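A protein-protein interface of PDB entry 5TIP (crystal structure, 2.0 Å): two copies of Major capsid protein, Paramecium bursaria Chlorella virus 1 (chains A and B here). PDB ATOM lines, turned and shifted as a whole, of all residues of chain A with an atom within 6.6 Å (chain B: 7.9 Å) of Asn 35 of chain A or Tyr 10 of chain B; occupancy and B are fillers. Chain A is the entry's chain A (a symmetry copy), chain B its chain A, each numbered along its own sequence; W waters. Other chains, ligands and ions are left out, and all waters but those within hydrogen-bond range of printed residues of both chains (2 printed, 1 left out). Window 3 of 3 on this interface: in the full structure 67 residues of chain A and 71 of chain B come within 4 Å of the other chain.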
ATOM      1  N   TYR A  33     -17.649   5.684  21.480  1.00  0.00           N
ATOM      2  CA  TYR A  33     -18.871   5.975  20.746  1.00  0.00           C
ATOM      3  C   TYR A  33     -19.143   7.475  20.769  1.00  0.00           C
ATOM      4  O   TYR A  33     -18.426   8.253  21.403  1.00  0.00           O
ATOM      5  CB  TYR A  33     -20.048   5.199  21.341  1.00  0.00           C
ATOM      6  CG  TYR A  33     -20.233   5.420  22.827  1.00  0.00           C
ATOM      7  CD1 TYR A  33     -19.527   4.666  23.757  1.00  0.00           C
ATOM      8  CD2 TYR A  33     -21.115   6.381  23.302  1.00  0.00           C
ATOM      9  CE1 TYR A  33     -19.692   4.867  25.113  1.00  0.00           C
ATOM     10  CE2 TYR A  33     -21.288   6.586  24.656  1.00  0.00           C
ATOM     11  CZ  TYR A  33     -20.574   5.827  25.558  1.00  0.00           C
ATOM     12  OH  TYR A  33     -20.745   6.032  26.908  1.00  0.00           O
ATOM     13  N   THR A  34     -20.191   7.882  20.057  1.00  0.00           N
ATOM     14  CA  THR A  34     -20.601   9.278  20.051  1.00  0.00           C
ATOM     15  C   THR A  34     -21.436   9.582  21.286  1.00  0.00           C
ATOM     16  O   THR A  34     -22.312   8.802  21.669  1.00  0.00           O
ATOM     17  CB  THR A  34     -21.401   9.601  18.787  1.00  0.00           C
ATOM     18  OG1 THR A  34     -22.519   8.711  18.685  1.00  0.00           O
ATOM     19  CG2 THR A  34     -20.532   9.457  17.550  1.00  0.00           C
ATOM     20  N   ASN A  35     -21.160  10.726  21.908  1.00  0.00           N
ATOM     21  CA  ASN A  35     -21.893  11.121  23.102  1.00  0.00           C
ATOM     22  C   ASN A  35     -23.361  11.357  22.769  1.00  0.00           C
ATOM     23  O   ASN A  35     -23.695  11.930  21.728  1.00  0.00           O
ATOM     24  CB  ASN A  35     -21.273  12.379  23.708  1.00  0.00           C
ATOM     25  CG  ASN A  35     -21.892  12.748  25.039  1.00  0.00           C
ATOM     26  OD1 ASN A  35     -22.420  11.893  25.749  1.00  0.00           O
ATOM     27  ND2 ASN A  35     -21.827  14.028  25.386  1.00  0.00           N
ATOM     28  N   PHE A  36     -24.244  10.913  23.661  1.00  0.00           N
ATOM     29  CA  PHE A  36     -25.680  11.058  23.456  1.00  0.00           C
ATOM     30  C   PHE A  36     -26.374  11.056  24.814  1.00  0.00           C
ATOM     31  O   PHE A  36     -25.742  10.882  25.860  1.00  0.00           O
ATOM     32  CB  PHE A  36     -26.231   9.950  22.553  1.00  0.00           C
ATOM     33  CG  PHE A  36     -26.226   8.588  23.191  1.00  0.00           C
ATOM     34  CD1 PHE A  36     -25.093   7.795  23.150  1.00  0.00           C
ATOM     35  CD2 PHE A  36     -27.354   8.103  23.834  1.00  0.00           C
ATOM     36  CE1 PHE A  36     -25.086   6.543  23.736  1.00  0.00           C
ATOM     37  CE2 PHE A  36     -27.351   6.854  24.424  1.00  0.00           C
ATOM     38  CZ  PHE A  36     -26.217   6.073  24.373  1.00  0.00           C
ATOM     39  N   ALA A  37     -27.690  11.255  24.785  1.00  0.00           N
ATOM     40  CA  ALA A  37     -28.520  11.184  25.978  1.00  0.00           C
ATOM     41  C   ALA A  37     -29.918  10.741  25.572  1.00  0.00           C
ATOM     42  O   ALA A  37     -30.381  11.040  24.468  1.00  0.00           O
ATOM     43  CB  ALA A  37     -28.578  12.528  26.711  1.00  0.00           C
ATOM     44  N   PHE A 209     -30.752  12.570  22.213  1.00  0.00           N
ATOM     45  CA  PHE A 209     -30.144  13.885  22.057  1.00  0.00           C
ATOM     46  C   PHE A 209     -28.681  13.702  21.676  1.00  0.00           C
ATOM     47  O   PHE A 209     -27.916  13.081  22.419  1.00  0.00           O
ATOM     48  CB  PHE A 209     -30.283  14.703  23.342  1.00  0.00           C
ATOM     49  CG  PHE A 209     -31.710  14.965  23.738  1.00  0.00           C
ATOM     50  CD1 PHE A 209     -32.428  14.029  24.461  1.00  0.00           C
ATOM     51  CD2 PHE A 209     -32.334  16.147  23.379  1.00  0.00           C
ATOM     52  CE1 PHE A 209     -33.741  14.265  24.819  1.00  0.00           C
ATOM     53  CE2 PHE A 209     -33.648  16.390  23.736  1.00  0.00           C
ATOM     54  CZ  PHE A 209     -34.350  15.448  24.457  1.00  0.00           C
ATOM     55  N   LEU A 210     -28.298  14.245  20.525  1.00  0.00           N
ATOM     56  CA  LEU A 210     -26.978  14.037  19.951  1.00  0.00           C
ATOM     57  C   LEU A 210     -26.074  15.245  20.173  1.00  0.00           C
ATOM     58  O   LEU A 210     -26.532  16.366  20.400  1.00  0.00           O
ATOM     59  CB  LEU A 210     -27.087  13.739  18.453  1.00  0.00           C
ATOM     60  CG  LEU A 210     -27.856  12.469  18.082  1.00  0.00           C
ATOM     61  CD1 LEU A 210     -28.037  12.367  16.575  1.00  0.00           C
ATOM     62  CD2 LEU A 210     -27.150  11.238  18.626  1.00  0.00           C
ATOM     63  N   ASP A 211     -24.769  14.989  20.105  1.00  0.00           N
ATOM     64  CA  ASP A 211     -23.758  16.026  20.223  1.00  0.00           C
ATOM     65  C   ASP A 211     -23.684  16.844  18.932  1.00  0.00           C
ATOM     66  O   ASP A 211     -24.280  16.495  17.911  1.00  0.00           O
ATOM     67  CB  ASP A 211     -22.400  15.411  20.558  1.00  0.00           C
ATOM     68  CG  ASP A 211     -21.544  16.319  21.423  1.00  0.00           C
ATOM     69  OD1 ASP A 211     -21.652  17.554  21.276  1.00  0.00           O
ATOM     70  OD2 ASP A 211     -20.769  15.797  22.253  1.00  0.00           O
ATOM     71  N   GLU A 214     -22.316  15.097  15.390  1.00  0.00           N
ATOM     72  CA  GLU A 214     -23.225  14.098  14.843  1.00  0.00           C
ATOM     73  C   GLU A 214     -24.586  14.707  14.538  1.00  0.00           C
ATOM     74  O   GLU A 214     -25.313  14.196  13.679  1.00  0.00           O
ATOM     75  CB  GLU A 214     -23.358  12.931  15.821  1.00  0.00           C
ATOM     76  CG  GLU A 214     -23.878  11.649  15.206  1.00  0.00           C
ATOM     77  CD  GLU A 214     -24.014  10.538  16.226  1.00  0.00           C
ATOM     78  OE1 GLU A 214     -24.067  10.843  17.438  1.00  0.00           O
ATOM     79  OE2 GLU A 214     -24.063   9.359  15.817  1.00  0.00           O
ATOM     80  N   SER B   5     -29.547  18.741  28.966  1.00  0.00           N
ATOM     81  CA  SER B   5     -28.682  19.156  30.067  1.00  0.00           C
ATOM     82  C   SER B   5     -27.679  18.078  30.461  1.00  0.00           C
ATOM     83  O   SER B   5     -26.639  18.401  31.042  1.00  0.00           O
ATOM     84  CB  SER B   5     -29.517  19.545  31.283  1.00  0.00           C
ATOM     85  OG  SER B   5     -28.679  20.082  32.292  1.00  0.00           O
ATOM     86  N   GLN B   6     -27.960  16.808  30.153  1.00  0.00           N
ATOM     87  CA  GLN B   6     -27.009  15.743  30.451  1.00  0.00           C
ATOM     88  C   GLN B   6     -25.838  15.755  29.478  1.00  0.00           C
ATOM     89  O   GLN B   6     -24.721  15.378  29.853  1.00  0.00           O
ATOM     90  CB  GLN B   6     -27.716  14.387  30.440  1.00  0.00           C
ATOM     91  CG  GLN B   6     -26.803  13.203  30.724  1.00  0.00           C
ATOM     92  CD  GLN B   6     -27.544  11.882  30.771  1.00  0.00           C
ATOM     93  OE1 GLN B   6     -28.579  11.756  31.428  1.00  0.00           O
ATOM     94  NE2 GLN B   6     -27.019  10.887  30.065  1.00  0.00           N
ATOM     95  N   LEU B   7     -26.073  16.180  28.234  1.00  0.00           N
ATOM     96  CA  LEU B   7     -24.983  16.286  27.271  1.00  0.00           C
ATOM     97  C   LEU B   7     -23.945  17.303  27.726  1.00  0.00           C
ATOM     98  O   LEU B   7     -22.739  17.089  27.560  1.00  0.00           O
ATOM     99  CB  LEU B   7     -25.532  16.663  25.894  1.00  0.00           C
ATOM    100  CG  LEU B   7     -26.194  15.540  25.099  1.00  0.00           C
ATOM    101  CD1 LEU B   7     -26.687  16.056  23.755  1.00  0.00           C
ATOM    102  CD2 LEU B   7     -25.225  14.384  24.921  1.00  0.00           C
ATOM    103  N   VAL B   8     -24.395  18.419  28.311  1.00  0.00           N
ATOM    104  CA  VAL B   8     -23.461  19.437  28.775  1.00  0.00           C
ATOM    105  C   VAL B   8     -22.681  18.964  29.994  1.00  0.00           C
ATOM    106  O   VAL B   8     -21.568  19.444  30.235  1.00  0.00           O
ATOM    107  CB  VAL B   8     -24.207  20.750  29.072  1.00  0.00           C
ATOM    108  CG1 VAL B   8     -23.223  21.906  29.211  1.00  0.00           C
ATOM    109  CG2 VAL B   8     -25.221  21.039  27.979  1.00  0.00           C
ATOM    110  N   ALA B   9     -23.225  18.021  30.766  1.00  0.00           N
ATOM    111  CA  ALA B   9     -22.501  17.433  31.892  1.00  0.00           C
ATOM    112  C   ALA B   9     -21.394  16.553  31.322  1.00  0.00           C
ATOM    113  O   ALA B   9     -21.475  15.322  31.293  1.00  0.00           O
ATOM    114  CB  ALA B   9     -23.443  16.644  32.794  1.00  0.00           C
ATOM    115  N   TYR B  10     -20.334  17.210  30.861  1.00  0.00           N
ATOM    116  CA  TYR B  10     -19.223  16.561  30.180  1.00  0.00           C
ATOM    117  C   TYR B  10     -17.937  16.874  30.931  1.00  0.00           C
ATOM    118  O   TYR B  10     -17.680  18.036  31.266  1.00  0.00           O
ATOM    119  CB  TYR B  10     -19.131  17.031  28.725  1.00  0.00           C
ATOM    120  CG  TYR B  10     -18.462  16.049  27.792  1.00  0.00           C
ATOM    121  CD1 TYR B  10     -19.156  14.958  27.285  1.00  0.00           C
ATOM    122  CD2 TYR B  10     -17.137  16.216  27.410  1.00  0.00           C
ATOM    123  CE1 TYR B  10     -18.550  14.060  26.428  1.00  0.00           C
ATOM    124  CE2 TYR B  10     -16.522  15.323  26.553  1.00  0.00           C
ATOM    125  CZ  TYR B  10     -17.233  14.246  26.065  1.00  0.00           C
ATOM    126  OH  TYR B  10     -16.625  13.353  25.212  1.00  0.00           O
ATOM    127  N   GLY B  11     -17.135  15.845  31.193  1.00  0.00           N
ATOM    128  CA  GLY B  11     -15.920  16.032  31.962  1.00  0.00           C
ATOM    129  C   GLY B  11     -14.689  15.380  31.370  1.00  0.00           C
ATOM    130  O   GLY B  11     -14.730  14.847  30.257  1.00  0.00           O
ATOM    131  N   ALA B  12     -13.579  15.423  32.111  1.00  0.00           N
ATOM    132  CA  ALA B  12     -12.330  14.845  31.628  1.00  0.00           C
ATOM    133  C   ALA B  12     -12.367  13.325  31.609  1.00  0.00           C
ATOM    134  O   ALA B  12     -11.577  12.707  30.887  1.00  0.00           O
ATOM    135  CB  ALA B  12     -11.159  15.329  32.484  1.00  0.00           C
ATOM    136  N   GLN B  13     -13.258  12.710  32.388  1.00  0.00           N
ATOM    137  CA  GLN B  13     -13.370  11.258  32.403  1.00  0.00           C
ATOM    138  C   GLN B  13     -14.066  10.720  31.163  1.00  0.00           C
ATOM    139  O   GLN B  13     -13.936   9.528  30.864  1.00  0.00           O
ATOM    140  CB  GLN B  13     -14.114  10.799  33.659  1.00  0.00           C
ATOM    141  CG  GLN B  13     -13.719  11.557  34.914  1.00  0.00           C
ATOM    142  CD  GLN B  13     -14.301  10.949  36.173  1.00  0.00           C
ATOM    143  OE1 GLN B  13     -14.572   9.751  36.228  1.00  0.00           O
ATOM    144  NE2 GLN B  13     -14.502  11.775  37.192  1.00  0.00           N
ATOM    145  N   ASP B  14     -14.797  11.567  30.438  1.00  0.00           N
ATOM    146  CA  ASP B  14     -15.472  11.166  29.208  1.00  0.00           C
ATOM    147  C   ASP B  14     -14.511  10.943  28.051  1.00  0.00           C
ATOM    148  O   ASP B  14     -14.954  10.527  26.974  1.00  0.00           O
ATOM    149  CB  ASP B  14     -16.509  12.217  28.819  1.00  0.00           C
ATOM    150  CG  ASP B  14     -17.605  12.355  29.849  1.00  0.00           C
ATOM    151  OD1 ASP B  14     -18.077  11.314  30.353  1.00  0.00           O
ATOM    152  OD2 ASP B  14     -17.988  13.501  30.162  1.00  0.00           O
ATOM    153  N   VAL B  15     -13.218  11.214  28.240  1.00  0.00           N
ATOM    154  CA  VAL B  15     -12.250  11.023  27.167  1.00  0.00           C
ATOM    155  C   VAL B  15     -12.122   9.545  26.818  1.00  0.00           C
ATOM    156  O   VAL B  15     -12.068   9.174  25.639  1.00  0.00           O
ATOM    157  CB  VAL B  15     -10.896  11.635  27.567  1.00  0.00           C
ATOM    158  CG1 VAL B  15      -9.786  11.072  26.710  1.00  0.00           C
ATOM    159  CG2 VAL B  15     -10.944  13.149  27.440  1.00  0.00           C
ATOM    160  N   TYR B  16     -12.078   8.678  27.831  1.00  0.00           N
ATOM    161  CA  TYR B  16     -11.985   7.242  27.595  1.00  0.00           C
ATOM    162  C   TYR B  16     -13.247   6.655  26.976  1.00  0.00           C
ATOM    163  O   TYR B  16     -13.204   5.519  26.492  1.00  0.00           O
ATOM    164  CB  TYR B  16     -11.688   6.512  28.907  1.00  0.00           C
ATOM    165  CG  TYR B  16     -10.279   6.695  29.416  1.00  0.00           C
ATOM    166  CD1 TYR B  16      -9.953   7.763  30.241  1.00  0.00           C
ATOM    167  CD2 TYR B  16      -9.276   5.797  29.079  1.00  0.00           C
ATOM    168  CE1 TYR B  16      -8.665   7.933  30.713  1.00  0.00           C
ATOM    169  CE2 TYR B  16      -7.985   5.959  29.544  1.00  0.00           C
ATOM    170  CZ  TYR B  16      -7.684   7.028  30.361  1.00  0.00           C
ATOM    171  OH  TYR B  16      -6.398   7.193  30.826  1.00  0.00           O
ATOM    172  N   LEU B  17     -14.357   7.389  26.972  1.00  0.00           N
ATOM    173  CA  LEU B  17     -15.634   6.863  26.507  1.00  0.00           C
ATOM    174  C   LEU B  17     -16.084   7.437  25.172  1.00  0.00           C
ATOM    175  O   LEU B  17     -16.487   6.679  24.284  1.00  0.00           O
ATOM    176  CB  LEU B  17     -16.716   7.116  27.566  1.00  0.00           C
ATOM    177  CG  LEU B  17     -16.475   6.484  28.936  1.00  0.00           C
ATOM    178  CD1 LEU B  17     -17.609   6.826  29.885  1.00  0.00           C
ATOM    179  CD2 LEU B  17     -16.317   4.980  28.809  1.00  0.00           C
ATOM    180  N   THR B  18     -16.034   8.759  24.998  1.00  0.00           N
ATOM    181  CA  THR B  18     -16.594   9.385  23.807  1.00  0.00           C
ATOM    182  C   THR B  18     -15.624  10.312  23.077  1.00  0.00           C
ATOM    183  O   THR B  18     -16.038  10.980  22.122  1.00  0.00           O
ATOM    184  CB  THR B  18     -17.865  10.166  24.161  1.00  0.00           C
ATOM    185  OG1 THR B  18     -17.593  11.058  25.248  1.00  0.00           O
ATOM    186  CG2 THR B  18     -18.978   9.216  24.564  1.00  0.00           C
ATOM    187  N   GLY B  19     -14.357  10.374  23.485  1.00  0.00           N
ATOM    188  CA  GLY B  19     -13.389  11.203  22.779  1.00  0.00           C
ATOM    189  C   GLY B  19     -12.941  10.555  21.484  1.00  0.00           C
ATOM    190  O   GLY B  19     -12.527   9.390  21.469  1.00  0.00           O
ATOM    191  N   ASN B  20     -13.006  11.324  20.391  1.00  0.00           N
ATOM    192  CA  ASN B  20     -12.748  10.798  19.055  1.00  0.00           C
ATOM    193  C   ASN B  20     -13.546   9.517  18.853  1.00  0.00           C
ATOM    194  O   ASN B  20     -12.958   8.428  18.846  1.00  0.00           O
ATOM    195  CB  ASN B  20     -11.264  10.544  18.813  1.00  0.00           C
ATOM    196  CG  ASN B  20     -10.491  11.821  18.601  1.00  0.00           C
ATOM    197  OD1 ASN B  20      -9.461  12.054  19.236  1.00  0.00           O
ATOM    198  ND2 ASN B  20     -10.998  12.672  17.723  1.00  0.00           N
ATOM    199  N   PRO B  21     -14.871   9.591  18.731  1.00  0.00           N
ATOM    200  CA  PRO B  21     -15.662   8.366  18.582  1.00  0.00           C
ATOM    201  C   PRO B  21     -15.141   7.505  17.444  1.00  0.00           C
ATOM    202  O   PRO B  21     -14.661   8.004  16.423  1.00  0.00           O
ATOM    203  CB  PRO B  21     -17.069   8.887  18.289  1.00  0.00           C
ATOM    204  CG  PRO B  21     -17.094  10.215  18.932  1.00  0.00           C
ATOM    205  CD  PRO B  21     -15.723  10.790  18.715  1.00  0.00           C
ATOM    206  N   ILE B  23     -17.110   4.388  16.847  1.00  0.00           N
ATOM    207  CA  ILE B  23     -18.361   3.776  16.438  1.00  0.00           C
ATOM    208  C   ILE B  23     -19.504   4.712  16.816  1.00  0.00           C
ATOM    209  O   ILE B  23     -19.320   5.718  17.502  1.00  0.00           O
ATOM    210  CB  ILE B  23     -18.563   2.394  17.090  1.00  0.00           C
ATOM    211  CG1 ILE B  23     -18.753   2.549  18.602  1.00  0.00           C
ATOM    212  CG2 ILE B  23     -17.386   1.499  16.814  1.00  0.00           C
ATOM    213  CD1 ILE B  23     -19.173   1.279  19.308  1.00  0.00           C
ATOM    214  N   THR B  24     -20.699   4.361  16.351  1.00  0.00           N
ATOM    215  CA  THR B  24     -21.935   5.012  16.758  1.00  0.00           C
ATOM    216  C   THR B  24     -23.014   3.948  16.874  1.00  0.00           C
ATOM    217  O   THR B  24     -23.024   2.973  16.118  1.00  0.00           O
ATOM    218  CB  THR B  24     -22.365   6.112  15.772  1.00  0.00           C
ATOM    219  OG1 THR B  24     -23.641   6.644  16.156  1.00  0.00           O
ATOM    220  CG2 THR B  24     -22.442   5.559  14.359  1.00  0.00           C
ATOM    221  N   PHE B  25     -23.914   4.131  17.834  1.00  0.00           N
ATOM    222  CA  PHE B  25     -24.958   3.147  18.091  1.00  0.00           C
ATOM    223  C   PHE B  25     -26.227   3.386  17.288  1.00  0.00           C
ATOM    224  O   PHE B  25     -27.142   2.557  17.348  1.00  0.00           O
ATOM    225  CB  PHE B  25     -25.314   3.118  19.580  1.00  0.00           C
ATOM    226  CG  PHE B  25     -24.197   2.647  20.465  1.00  0.00           C
ATOM    227  CD1 PHE B  25     -23.744   1.340  20.394  1.00  0.00           C
ATOM    228  CD2 PHE B  25     -23.622   3.501  21.391  1.00  0.00           C
ATOM    229  CE1 PHE B  25     -22.724   0.901  21.214  1.00  0.00           C
ATOM    230  CE2 PHE B  25     -22.605   3.066  22.215  1.00  0.00           C
ATOM    231  CZ  PHE B  25     -22.155   1.766  22.126  1.00  0.00           C
ATOM    232  N   PHE B  26     -26.315   4.489  16.545  1.00  0.00           N
ATOM    233  CA  PHE B  26     -27.565   4.886  15.907  1.00  0.00           C
ATOM    234  C   PHE B  26     -27.476   4.888  14.385  1.00  0.00           C
ATOM    235  O   PHE B  26     -28.282   5.548  13.722  1.00  0.00           O
ATOM    236  CB  PHE B  26     -28.007   6.258  16.417  1.00  0.00           C
ATOM    237  CG  PHE B  26     -28.000   6.379  17.913  1.00  0.00           C
ATOM    238  CD1 PHE B  26     -28.992   5.783  18.671  1.00  0.00           C
ATOM    239  CD2 PHE B  26     -27.007   7.092  18.559  1.00  0.00           C
ATOM    240  CE1 PHE B  26     -28.990   5.890  20.048  1.00  0.00           C
ATOM    241  CE2 PHE B  26     -27.001   7.205  19.936  1.00  0.00           C
ATOM    242  CZ  PHE B  26     -27.994   6.602  20.681  1.00  0.00           C
HETATM  243  O   HOH W   1     -24.449  12.059  28.191  1.00  0.00           O
HETATM  244  O   HOH W   2     -18.672  12.378  20.897  1.00  0.00           O
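Water W1 lies within hydrogen-bond range of O of Phe 36 of chain A, OD1 of Asn 35 of chain A and NE2 of Gln 6 of chain B. Water W2 bridges the backbone NH (N) of Asn 35 of chain A (3.2 Å) and the backbone carbonyl oxygen (O) of Thr 18 of chain B (3.2 Å).
Of the printed residues of chain B, Tyr 33 of chain A touches Leu 17, Thr 18, Pro 21, Ile 23 and Phe 25. Printed residues of chain B within 4 Å of Thr 34 of chain A: Pro 21, Ile 23 and Thr 24. Of chain B, only Leu 7, Tyr 10 and Thr 18 come within 4 Å of Asn 35 of chain A. Tyr 10 of chain B touches just one residue of chain A: Asn 35 (3.4 Å). Of the printed residues of chain A, Phe 26 of chain B touches Phe 36. The nearest residue of chain B that does not touch Asn 35 of chain A is Pro 21 of chain B (5.1 Å). The nearest residue of chain A that does not touch Tyr 10 of chain B is Asp 211 of chain A (5.0 Å). The nearest printed residue of chain B that does not touch Glu 214 of chain A is Phe 26 of chain B (4.6 Å).
Of the 9 printed residues of chain A, 8 touch a printed residue of chain B. Hydrophobic or aromatic side chains of chain A within 4 Å of the printed part of chain B: Tyr 33, Phe 36 and Phe 209. Hydrophobic or aromatic side chains of chain B within 4 Å of the printed part of chain A: Leu 7, Tyr 10, Pro 21, Phe 25 and Phe 26. Among the printed residues, 17 pairs touch across the chains. Among the printed residues, no Asp or Glu carboxylate lies within 4 Å of a Lys or Arg side-chain nitrogen of the other chain.
Among the printed residues, merely in contact across the chains: Tyr 33 of chain A with Thr 18 of chain B, Tyr 33 of chain A with Pro 21 of chain B, Tyr 33 of chain A with Ile 23 of chain B, Tyr 33 of chain A with Phe 25 of chain B, Thr 34 of chain A with Pro 21 of chain B, Asn 35 of chain A with Leu 7 of chain B, Asn 35 of chain A with Tyr 10 of chain B, Asn 35 of chain A with Thr 18 of chain B, Phe 36 of chain A with Leu 7 of chain B, Phe 36 of chain A with Phe 26 of chain B, Ala 37 of chain A with Leu 7 of chain B, Phe 209 of chain A with Leu 7 of chain B and Leu 210 of chain A with Leu 7 of chain B.
The side-chain hydroxyl of Thr 18 of chain B sits at hydrogen-bond distance from the side-chain hydroxyl of Tyr 10 of chain B, at 2.5 Å. The backbone carbonyl oxygen of Asp 14 of chain B sits at hydrogen-bond distance from the side-chain hydroxyl of Thr 18 of chain B, at 3.2 Å. N of Phe 26 of chain B lies close to OG1 of Thr 24 of chain B. The side-chain hydroxyl of Thr 34 of chain A lies within hydrogen-bond range of the side-chain carboxylate of Glu 214 of chain A, at 2.9 Å. The backbone NH (N) of Phe 209 of chain A lies within hydrogen-bond range of the backbone carbonyl oxygen (O) of Ala 37 of chain A.
The backbone carbonyl oxygen of Leu 17 of chain B sits at hydrogen-bond distance from the backbone NH of Tyr 33 of chain A (3.2 Å). The backbone carbonyl oxygen of Ile 23 of chain B is in hydrogen-bond range of the backbone NH of Thr 34 of chain A (3.5 Å). The side-chain hydroxyl (OG1) of Thr 24 of chain B is in hydrogen-bond range of the side-chain hydroxyl (OG1) of Thr 34 of chain A (3.5 Å). The side-chain hydroxyl of Thr 24 of chain B sits at hydrogen-bond distance from the side-chain carboxylate of Glu 214 of chain A (2.8 Å).
No position is printed for both chains.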
